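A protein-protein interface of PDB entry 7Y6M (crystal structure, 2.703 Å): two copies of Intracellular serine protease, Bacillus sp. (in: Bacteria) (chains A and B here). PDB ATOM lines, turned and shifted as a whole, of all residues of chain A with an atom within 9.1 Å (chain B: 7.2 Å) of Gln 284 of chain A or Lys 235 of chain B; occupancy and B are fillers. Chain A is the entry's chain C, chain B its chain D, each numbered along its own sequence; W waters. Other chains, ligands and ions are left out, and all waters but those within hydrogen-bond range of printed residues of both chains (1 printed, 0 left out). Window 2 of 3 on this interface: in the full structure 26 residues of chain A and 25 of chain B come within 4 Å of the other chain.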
ATOM      1  N   LYS A 276     -16.627 -15.806  28.440  1.00  0.00           N
ATOM      2  CA  LYS A 276     -15.197 -16.069  28.528  1.00  0.00           C
ATOM      3  C   LYS A 276     -14.632 -16.502  27.171  1.00  0.00           C
ATOM      4  O   LYS A 276     -13.545 -16.054  26.760  1.00  0.00           O
ATOM      5  CB  LYS A 276     -14.935 -17.129  29.596  1.00  0.00           C
ATOM      6  CG  LYS A 276     -13.843 -16.748  30.588  1.00  0.00           C
ATOM      7  CD  LYS A 276     -13.653 -17.814  31.656  1.00  0.00           C
ATOM      8  CE  LYS A 276     -12.615 -17.422  32.695  1.00  0.00           C
ATOM      9  NZ  LYS A 276     -11.229 -17.471  32.173  1.00  0.00           N
ATOM     10  N   ASN A 277     -15.385 -17.337  26.439  1.00  0.00           N
ATOM     11  CA  ASN A 277     -14.945 -17.762  25.114  1.00  0.00           C
ATOM     12  C   ASN A 277     -14.848 -16.585  24.152  1.00  0.00           C
ATOM     13  O   ASN A 277     -13.855 -16.430  23.433  1.00  0.00           O
ATOM     14  CB  ASN A 277     -15.911 -18.798  24.552  1.00  0.00           C
ATOM     15  CG  ASN A 277     -15.582 -20.205  24.985  1.00  0.00           C
ATOM     16  OD1 ASN A 277     -16.428 -21.089  24.872  1.00  0.00           O
ATOM     17  ND2 ASN A 277     -14.359 -20.430  25.472  1.00  0.00           N
ATOM     18  N   ALA A 278     -15.899 -15.765  24.104  1.00  0.00           N
ATOM     19  CA  ALA A 278     -15.934 -14.621  23.199  1.00  0.00           C
ATOM     20  C   ALA A 278     -14.853 -13.600  23.520  1.00  0.00           C
ATOM     21  O   ALA A 278     -14.347 -12.923  22.615  1.00  0.00           O
ATOM     22  CB  ALA A 278     -17.308 -13.949  23.259  1.00  0.00           C
ATOM     23  N   GLU A 279     -14.492 -13.462  24.790  1.00  0.00           N
ATOM     24  CA  GLU A 279     -13.602 -12.373  25.144  1.00  0.00           C
ATOM     25  C   GLU A 279     -12.145 -12.786  25.138  1.00  0.00           C
ATOM     26  O   GLU A 279     -11.280 -11.959  24.830  1.00  0.00           O
ATOM     27  CB  GLU A 279     -13.995 -11.805  26.503  1.00  0.00           C
ATOM     28  CG  GLU A 279     -15.349 -11.117  26.474  1.00  0.00           C
ATOM     29  CD  GLU A 279     -15.405  -9.945  25.498  1.00  0.00           C
ATOM     30  OE1 GLU A 279     -14.360  -9.504  24.979  1.00  0.00           O
ATOM     31  OE2 GLU A 279     -16.515  -9.451  25.245  1.00  0.00           O
ATOM     32  N   GLU A 280     -11.851 -14.049  25.447  1.00  0.00           N
ATOM     33  CA  GLU A 280     -10.470 -14.503  25.319  1.00  0.00           C
ATOM     34  C   GLU A 280     -10.031 -14.489  23.861  1.00  0.00           C
ATOM     35  O   GLU A 280      -8.860 -14.234  23.572  1.00  0.00           O
ATOM     36  CB  GLU A 280     -10.304 -15.882  25.972  1.00  0.00           C
ATOM     37  CG  GLU A 280      -9.975 -15.720  27.484  1.00  0.00           C
ATOM     38  CD  GLU A 280     -10.594 -16.747  28.418  1.00  0.00           C
ATOM     39  OE1 GLU A 280     -11.062 -17.806  27.937  1.00  0.00           O
ATOM     40  OE2 GLU A 280     -10.626 -16.459  29.641  1.00  0.00           O
ATOM     41  N   GLU A 281     -10.974 -14.676  22.931  1.00  0.00           N
ATOM     42  CA  GLU A 281     -10.657 -14.563  21.510  1.00  0.00           C
ATOM     43  C   GLU A 281     -10.436 -13.112  21.112  1.00  0.00           C
ATOM     44  O   GLU A 281      -9.462 -12.789  20.420  1.00  0.00           O
ATOM     45  CB  GLU A 281     -11.769 -15.176  20.653  1.00  0.00           C
ATOM     46  CG  GLU A 281     -11.493 -15.028  19.156  1.00  0.00           C
ATOM     47  CD  GLU A 281     -12.318 -15.966  18.296  1.00  0.00           C
ATOM     48  OE1 GLU A 281     -12.003 -17.184  18.240  1.00  0.00           O
ATOM     49  OE2 GLU A 281     -13.279 -15.475  17.663  1.00  0.00           O
ATOM     50  N   ALA A 282     -11.338 -12.224  21.530  1.00  0.00           N
ATOM     51  CA  ALA A 282     -11.240 -10.830  21.118  1.00  0.00           C
ATOM     52  C   ALA A 282     -10.009 -10.163  21.714  1.00  0.00           C
ATOM     53  O   ALA A 282      -9.385  -9.312  21.071  1.00  0.00           O
ATOM     54  CB  ALA A 282     -12.507 -10.078  21.522  1.00  0.00           C
ATOM     55  N   PHE A 283      -9.645 -10.534  22.940  1.00  0.00           N
ATOM     56  CA  PHE A 283      -8.510  -9.931  23.626  1.00  0.00           C
ATOM     57  C   PHE A 283      -7.227 -10.735  23.459  1.00  0.00           C
ATOM     58  O   PHE A 283      -6.148 -10.220  23.780  1.00  0.00           O
ATOM     59  CB  PHE A 283      -8.823  -9.752  25.127  1.00  0.00           C
ATOM     60  CG  PHE A 283      -9.643  -8.536  25.435  1.00  0.00           C
ATOM     61  CD1 PHE A 283      -9.049  -7.269  25.476  1.00  0.00           C
ATOM     62  CD2 PHE A 283     -10.996  -8.641  25.676  1.00  0.00           C
ATOM     63  CE1 PHE A 283      -9.797  -6.125  25.749  1.00  0.00           C
ATOM     64  CE2 PHE A 283     -11.750  -7.497  25.952  1.00  0.00           C
ATOM     65  CZ  PHE A 283     -11.144  -6.234  25.987  1.00  0.00           C
ATOM     66  N   GLN A 284      -7.328 -11.979  22.979  1.00  0.00           N
ATOM     67  CA  GLN A 284      -6.181 -12.819  22.642  1.00  0.00           C
ATOM     68  C   GLN A 284      -5.349 -13.183  23.870  1.00  0.00           C
ATOM     69  O   GLN A 284      -4.149 -13.426  23.762  1.00  0.00           O
ATOM     70  CB  GLN A 284      -5.305 -12.169  21.561  1.00  0.00           C
ATOM     71  CG  GLN A 284      -5.840 -12.329  20.108  1.00  0.00           C
ATOM     72  CD  GLN A 284      -5.571 -13.729  19.507  1.00  0.00           C
ATOM     73  OE1 GLN A 284      -5.626 -14.744  20.212  1.00  0.00           O
ATOM     74  NE2 GLN A 284      -5.278 -13.777  18.199  1.00  0.00           N
ATOM     75  N   ARG A 285      -5.988 -13.230  25.037  1.00  0.00           N
ATOM     76  CA  ARG A 285      -5.369 -13.683  26.281  1.00  0.00           C
ATOM     77  C   ARG A 285      -6.483 -14.173  27.197  1.00  0.00           C
ATOM     78  O   ARG A 285      -7.671 -13.992  26.906  1.00  0.00           O
ATOM     79  CB  ARG A 285      -4.562 -12.569  26.965  1.00  0.00           C
ATOM     80  CG  ARG A 285      -5.420 -11.416  27.422  1.00  0.00           C
ATOM     81  CD  ARG A 285      -4.800 -10.620  28.541  1.00  0.00           C
ATOM     82  NE  ARG A 285      -5.467  -9.331  28.689  1.00  0.00           N
ATOM     83  CZ  ARG A 285      -6.442  -9.075  29.560  1.00  0.00           C
ATOM     84  NH1 ARG A 285      -6.873 -10.020  30.391  1.00  0.00           N
ATOM     85  NH2 ARG A 285      -6.978  -7.860  29.610  1.00  0.00           N
ATOM     86  N   LYS A 286      -6.082 -14.789  28.313  1.00  0.00           N
ATOM     87  CA  LYS A 286      -7.043 -15.163  29.347  1.00  0.00           C
ATOM     88  C   LYS A 286      -7.502 -13.936  30.140  1.00  0.00           C
ATOM     89  O   LYS A 286      -6.709 -13.046  30.468  1.00  0.00           O
ATOM     90  CB  LYS A 286      -6.439 -16.198  30.299  1.00  0.00           C
ATOM     91  CG  LYS A 286      -6.252 -17.600  29.732  1.00  0.00           C
ATOM     92  CD  LYS A 286      -7.527 -18.161  29.116  1.00  0.00           C
ATOM     93  CE  LYS A 286      -7.611 -19.684  29.283  1.00  0.00           C
ATOM     94  NZ  LYS A 286      -8.264 -20.121  30.584  1.00  0.00           N
ATOM     95  N   LEU A 287      -8.792 -13.894  30.468  1.00  0.00           N
ATOM     96  CA  LEU A 287      -9.357 -12.748  31.163  1.00  0.00           C
ATOM     97  C   LEU A 287      -9.537 -13.033  32.653  1.00  0.00           C
ATOM     98  O   LEU A 287      -9.994 -14.110  33.046  1.00  0.00           O
ATOM     99  CB  LEU A 287     -10.686 -12.352  30.538  1.00  0.00           C
ATOM    100  CG  LEU A 287     -10.660 -11.039  29.766  1.00  0.00           C
ATOM    101  CD1 LEU A 287      -9.597 -11.096  28.711  1.00  0.00           C
ATOM    102  CD2 LEU A 287     -12.035 -10.735  29.138  1.00  0.00           C
ATOM    103  N   GLU A 291     -12.441  -8.796  35.200  1.00  0.00           N
ATOM    104  CA  GLU A 291     -12.668  -8.442  33.805  1.00  0.00           C
ATOM    105  C   GLU A 291     -13.895  -9.166  33.277  1.00  0.00           C
ATOM    106  O   GLU A 291     -14.785  -8.556  32.676  1.00  0.00           O
ATOM    107  CB  GLU A 291     -11.426  -8.759  32.963  1.00  0.00           C
ATOM    108  CG  GLU A 291     -10.290  -7.764  33.139  1.00  0.00           C
ATOM    109  CD  GLU A 291      -9.012  -8.191  32.431  1.00  0.00           C
ATOM    110  OE1 GLU A 291      -8.538  -9.309  32.660  1.00  0.00           O
ATOM    111  OE2 GLU A 291      -8.471  -7.409  31.634  1.00  0.00           O
ATOM    112  N   GLU B 204       3.299  -5.144  19.105  1.00  0.00           N
ATOM    113  CA  GLU B 204       2.990  -4.653  20.443  1.00  0.00           C
ATOM    114  C   GLU B 204       4.080  -3.707  20.936  1.00  0.00           C
ATOM    115  O   GLU B 204       5.268  -3.913  20.670  1.00  0.00           O
ATOM    116  CB  GLU B 204       2.802  -5.805  21.447  1.00  0.00           C
ATOM    117  CG  GLU B 204       2.041  -7.013  20.893  1.00  0.00           C
ATOM    118  CD  GLU B 204       1.572  -7.952  21.984  1.00  0.00           C
ATOM    119  OE1 GLU B 204       2.410  -8.674  22.566  1.00  0.00           O
ATOM    120  OE2 GLU B 204       0.357  -7.975  22.258  1.00  0.00           O
ATOM    121  N   GLU B 205       3.661  -2.659  21.642  1.00  0.00           N
ATOM    122  CA  GLU B 205       4.545  -1.711  22.299  1.00  0.00           C
ATOM    123  C   GLU B 205       4.095  -1.610  23.742  1.00  0.00           C
ATOM    124  O   GLU B 205       2.902  -1.433  24.000  1.00  0.00           O
ATOM    125  CB  GLU B 205       4.486  -0.332  21.640  1.00  0.00           C
ATOM    126  CG  GLU B 205       4.701  -0.359  20.149  1.00  0.00           C
ATOM    127  CD  GLU B 205       3.430  -0.599  19.343  1.00  0.00           C
ATOM    128  OE1 GLU B 205       2.307  -0.490  19.897  1.00  0.00           O
ATOM    129  OE2 GLU B 205       3.572  -0.901  18.138  1.00  0.00           O
ATOM    130  N   PHE B 206       5.034  -1.710  24.677  1.00  0.00           N
ATOM    131  CA  PHE B 206       4.699  -1.770  26.093  1.00  0.00           C
ATOM    132  C   PHE B 206       5.170  -0.521  26.818  1.00  0.00           C
ATOM    133  O   PHE B 206       6.348  -0.145  26.736  1.00  0.00           O
ATOM    134  CB  PHE B 206       5.310  -3.012  26.737  1.00  0.00           C
ATOM    135  CG  PHE B 206       4.841  -4.266  26.121  1.00  0.00           C
ATOM    136  CD1 PHE B 206       5.468  -4.769  24.988  1.00  0.00           C
ATOM    137  CD2 PHE B 206       3.738  -4.926  26.627  1.00  0.00           C
ATOM    138  CE1 PHE B 206       5.016  -5.948  24.388  1.00  0.00           C
ATOM    139  CE2 PHE B 206       3.275  -6.090  26.030  1.00  0.00           C
ATOM    140  CZ  PHE B 206       3.921  -6.606  24.909  1.00  0.00           C
ATOM    141  N   ALA B 211       0.775  -0.954  31.214  1.00  0.00           N
ATOM    142  CA  ALA B 211       0.838  -2.351  30.796  1.00  0.00           C
ATOM    143  C   ALA B 211       0.448  -3.338  31.893  1.00  0.00           C
ATOM    144  O   ALA B 211       0.121  -4.492  31.583  1.00  0.00           O
ATOM    145  CB  ALA B 211       2.254  -2.670  30.295  1.00  0.00           C
ATOM    146  N   ASN B 213      -1.848  -5.317  34.196  1.00  0.00           N
ATOM    147  CA  ASN B 213      -3.267  -5.628  34.090  1.00  0.00           C
ATOM    148  C   ASN B 213      -4.093  -4.781  35.053  1.00  0.00           C
ATOM    149  O   ASN B 213      -5.148  -4.265  34.678  1.00  0.00           O
ATOM    150  CB  ASN B 213      -3.483  -7.118  34.341  1.00  0.00           C
ATOM    151  CG  ASN B 213      -4.939  -7.510  34.331  1.00  0.00           C
ATOM    152  OD1 ASN B 213      -5.570  -7.669  35.390  1.00  0.00           O
ATOM    153  ND2 ASN B 213      -5.483  -7.688  33.139  1.00  0.00           N
ATOM    154  N   ALA B 233      -0.069  -0.578  21.278  1.00  0.00           N
ATOM    155  CA  ALA B 233      -0.947  -1.711  21.039  1.00  0.00           C
ATOM    156  C   ALA B 233      -0.465  -2.863  21.902  1.00  0.00           C
ATOM    157  O   ALA B 233       0.702  -3.250  21.809  1.00  0.00           O
ATOM    158  CB  ALA B 233      -0.946  -2.100  19.557  1.00  0.00           C
ATOM    159  N   ASN B 234      -1.346  -3.391  22.746  1.00  0.00           N
ATOM    160  CA  ASN B 234      -1.032  -4.625  23.455  1.00  0.00           C
ATOM    161  C   ASN B 234      -2.315  -5.252  23.988  1.00  0.00           C
ATOM    162  O   ASN B 234      -3.422  -4.756  23.764  1.00  0.00           O
ATOM    163  CB  ASN B 234      -0.016  -4.413  24.591  1.00  0.00           C
ATOM    164  CG  ASN B 234      -0.314  -3.206  25.447  1.00  0.00           C
ATOM    165  OD1 ASN B 234      -1.221  -3.218  26.279  1.00  0.00           O
ATOM    166  ND2 ASN B 234       0.485  -2.163  25.274  1.00  0.00           N
ATOM    167  N   LYS B 235      -2.153  -6.372  24.684  1.00  0.00           N
ATOM    168  CA  LYS B 235      -3.293  -7.096  25.207  1.00  0.00           C
ATOM    169  C   LYS B 235      -3.779  -6.547  26.551  1.00  0.00           C
ATOM    170  O   LYS B 235      -4.492  -7.252  27.278  1.00  0.00           O
ATOM    171  CB  LYS B 235      -2.945  -8.578  25.319  1.00  0.00           C
ATOM    172  CG  LYS B 235      -2.643  -9.249  23.989  1.00  0.00           C
ATOM    173  CD  LYS B 235      -2.043 -10.646  24.219  1.00  0.00           C
ATOM    174  CE  LYS B 235      -1.552 -11.306  22.936  1.00  0.00           C
ATOM    175  NZ  LYS B 235      -0.099 -11.048  22.757  1.00  0.00           N
ATOM    176  N   GLU B 236      -3.425  -5.306  26.890  1.00  0.00           N
ATOM    177  CA  GLU B 236      -3.806  -4.717  28.164  1.00  0.00           C
ATOM    178  C   GLU B 236      -4.330  -3.296  27.996  1.00  0.00           C
ATOM    179  O   GLU B 236      -4.174  -2.455  28.889  1.00  0.00           O
ATOM    180  CB  GLU B 236      -2.640  -4.749  29.150  1.00  0.00           C
ATOM    181  CG  GLU B 236      -2.204  -6.176  29.542  1.00  0.00           C
ATOM    182  CD  GLU B 236      -3.276  -6.994  30.248  1.00  0.00           C
ATOM    183  OE1 GLU B 236      -4.336  -6.438  30.616  1.00  0.00           O
ATOM    184  OE2 GLU B 236      -3.050  -8.204  30.444  1.00  0.00           O
ATOM    185  N   ILE B 237      -4.959  -3.012  26.869  1.00  0.00           N
ATOM    186  CA  ILE B 237      -5.688  -1.766  26.694  1.00  0.00           C
ATOM    187  C   ILE B 237      -7.129  -1.990  27.132  1.00  0.00           C
ATOM    188  O   ILE B 237      -7.793  -2.927  26.685  1.00  0.00           O
ATOM    189  CB  ILE B 237      -5.618  -1.291  25.232  1.00  0.00           C
ATOM    190  CG1 ILE B 237      -4.172  -1.298  24.726  1.00  0.00           C
ATOM    191  CG2 ILE B 237      -6.277   0.084  25.068  1.00  0.00           C
ATOM    192  CD1 ILE B 237      -3.348  -0.139  25.215  1.00  0.00           C
ATOM    193  N   ASP B 238      -7.622  -1.134  28.004  1.00  0.00           N
ATOM    194  CA  ASP B 238      -8.994  -1.297  28.454  1.00  0.00           C
ATOM    195  C   ASP B 238      -9.994  -0.497  27.629  1.00  0.00           C
ATOM    196  O   ASP B 238     -11.059  -1.021  27.297  1.00  0.00           O
ATOM    197  CB  ASP B 238      -9.090  -0.904  29.915  1.00  0.00           C
ATOM    198  CG  ASP B 238      -8.408  -1.892  30.800  1.00  0.00           C
ATOM    199  OD1 ASP B 238      -9.053  -2.905  31.125  1.00  0.00           O
ATOM    200  OD2 ASP B 238      -7.229  -1.659  31.147  1.00  0.00           O
ATOM    201  N   SER B 306      -9.227  -3.445  16.310  1.00  0.00           N
ATOM    202  CA  SER B 306      -8.711  -4.479  17.186  1.00  0.00           C
ATOM    203  C   SER B 306      -8.698  -4.005  18.638  1.00  0.00           C
ATOM    204  O   SER B 306      -8.382  -2.846  18.937  1.00  0.00           O
ATOM    205  CB  SER B 306      -7.302  -4.884  16.734  1.00  0.00           C
ATOM    206  OG  SER B 306      -6.702  -5.819  17.614  1.00  0.00           O
ATOM    207  N   LYS B 307      -9.072  -4.916  19.544  1.00  0.00           N
ATOM    208  CA  LYS B 307      -8.910  -4.647  20.966  1.00  0.00           C
ATOM    209  C   LYS B 307      -7.475  -4.276  21.299  1.00  0.00           C
ATOM    210  O   LYS B 307      -7.229  -3.613  22.312  1.00  0.00           O
ATOM    211  CB  LYS B 307      -9.308  -5.864  21.810  1.00  0.00           C
ATOM    212  CG  LYS B 307     -10.662  -6.458  21.535  1.00  0.00           C
ATOM    213  CD  LYS B 307     -11.763  -5.874  22.403  1.00  0.00           C
ATOM    214  CE  LYS B 307     -13.122  -6.317  21.862  1.00  0.00           C
ATOM    215  NZ  LYS B 307     -13.190  -6.073  20.373  1.00  0.00           N
ATOM    216  N   ALA B 308      -6.513  -4.721  20.488  1.00  0.00           N
ATOM    217  CA  ALA B 308      -5.117  -4.402  20.771  1.00  0.00           C
ATOM    218  C   ALA B 308      -4.875  -2.906  20.746  1.00  0.00           C
ATOM    219  O   ALA B 308      -4.006  -2.406  21.467  1.00  0.00           O
ATOM    220  CB  ALA B 308      -4.193  -5.085  19.769  1.00  0.00           C
HETATM  221  O   HOH W   1      -6.754  -8.025  20.364  1.00  0.00           O
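The backbone carbonyl oxygen (O) of Lys 235 of chain B sits at hydrogen-bond distance from the guanidinium group (NE) of Arg 285 of chain A, 2.7 Å away.
The side-chain carboxylate (OE1) of Glu 236 of chain B lies within salt-bridge range of the guanidinium group (NH2) of Arg 285 of chain A, at 3.2 Å.
ND2 of Asn 213 of chain B lies within hydrogen-bond range of OE2 of Glu 291 of chain A, at 3.4 Å.
N of Glu 236 of chain B lies within hydrogen-bond range of OD1 of Asn 234 of chain B (3.1 Å).
OE1 of Glu 236 of chain B lies within hydrogen-bond range of ND2 of Asn 213 of chain B (3.0 Å).
NH2 of Arg 285 of chain A is in salt-bridge range of OE2 of Glu 291 of chain A (2.6 Å).
The backbone carbonyl oxygen of Glu 280 of chain A is in hydrogen-bond range of the backbone NH of Arg 285 of chain A.
The side-chain amino group (NZ) of Lys 235 of chain B lies within salt-bridge range of the side-chain carboxylate (OE2) of Glu 204 of chain B (3.1 Å).
Among the printed residues, pairs that only touch across the chains: Ala 282 of chain A with Lys 307 of chain B, Gln 284 of chain A with Lys 235 of chain B, Phe 283 of chain A with Lys 235 of chain B, Phe 283 of chain A with Lys 307 of chain B, Arg 285 of chain A with Asn 213 of chain B and Phe 283 of chain A with Ile 237 of chain B.
Of the printed residues of chain B, Phe 283 of chain A touches Lys 235, Ile 237 and Lys 307.
Gln 284 of chain A touches just one residue of chain B: Lys 235 (3.5 Å).
Glu 204 of chain B touches none of the printed residues of chain A.
Printed residues of chain A within 4 Å of Asn 213 of chain B: Arg 285 and Glu 291.
No residue of chain A comes within 4 Å of Asn 234 of chain B.
Lys 235 of chain B touches just these residues of chain A: Phe 283 (3.6 Å), Gln 284 (3.5 Å) and Arg 285 (2.7 Å).
Of the printed residues of chain A, Lys 307 of chain B touches Ala 282 and Phe 283.
Ala 308 of chain B touches none of the printed residues of chain A.
The nearest printed residue of chain B that does not touch Ala 282 of chain A is Ala 308 of chain B (5.4 Å).
Printed residues of chain B that touch a printed residue of chain A: Asn 213, Lys 235, Glu 236, Ile 237 and Lys 307.
Of the 13 printed residues of chain A, 5 touch a printed residue of chain B.
Printed residues of chain A that touch a printed residue of chain B: Ala 282, Phe 283, Gln 284, Arg 285 and Glu 291.
Hydrophobic or aromatic side chains of chain A within 4 Å of the printed part of chain B: Ala 282 and Phe 283.
Among the printed residues, Asp or Glu carboxylates within 4 Å of a Lys or Arg side-chain nitrogen of the other chain: Arg 285 of chain A with Glu 236 of chain B.
No position is printed for both chains.
Of the 9 pairs that touch across the chains among the printed residues, none has its exchanged pair printed and touching as well.
Water W1 lies within hydrogen-bond range of O of Ala 282 of chain A (3.0 Å) and N of Ala 308 of chain B (3.3 Å).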
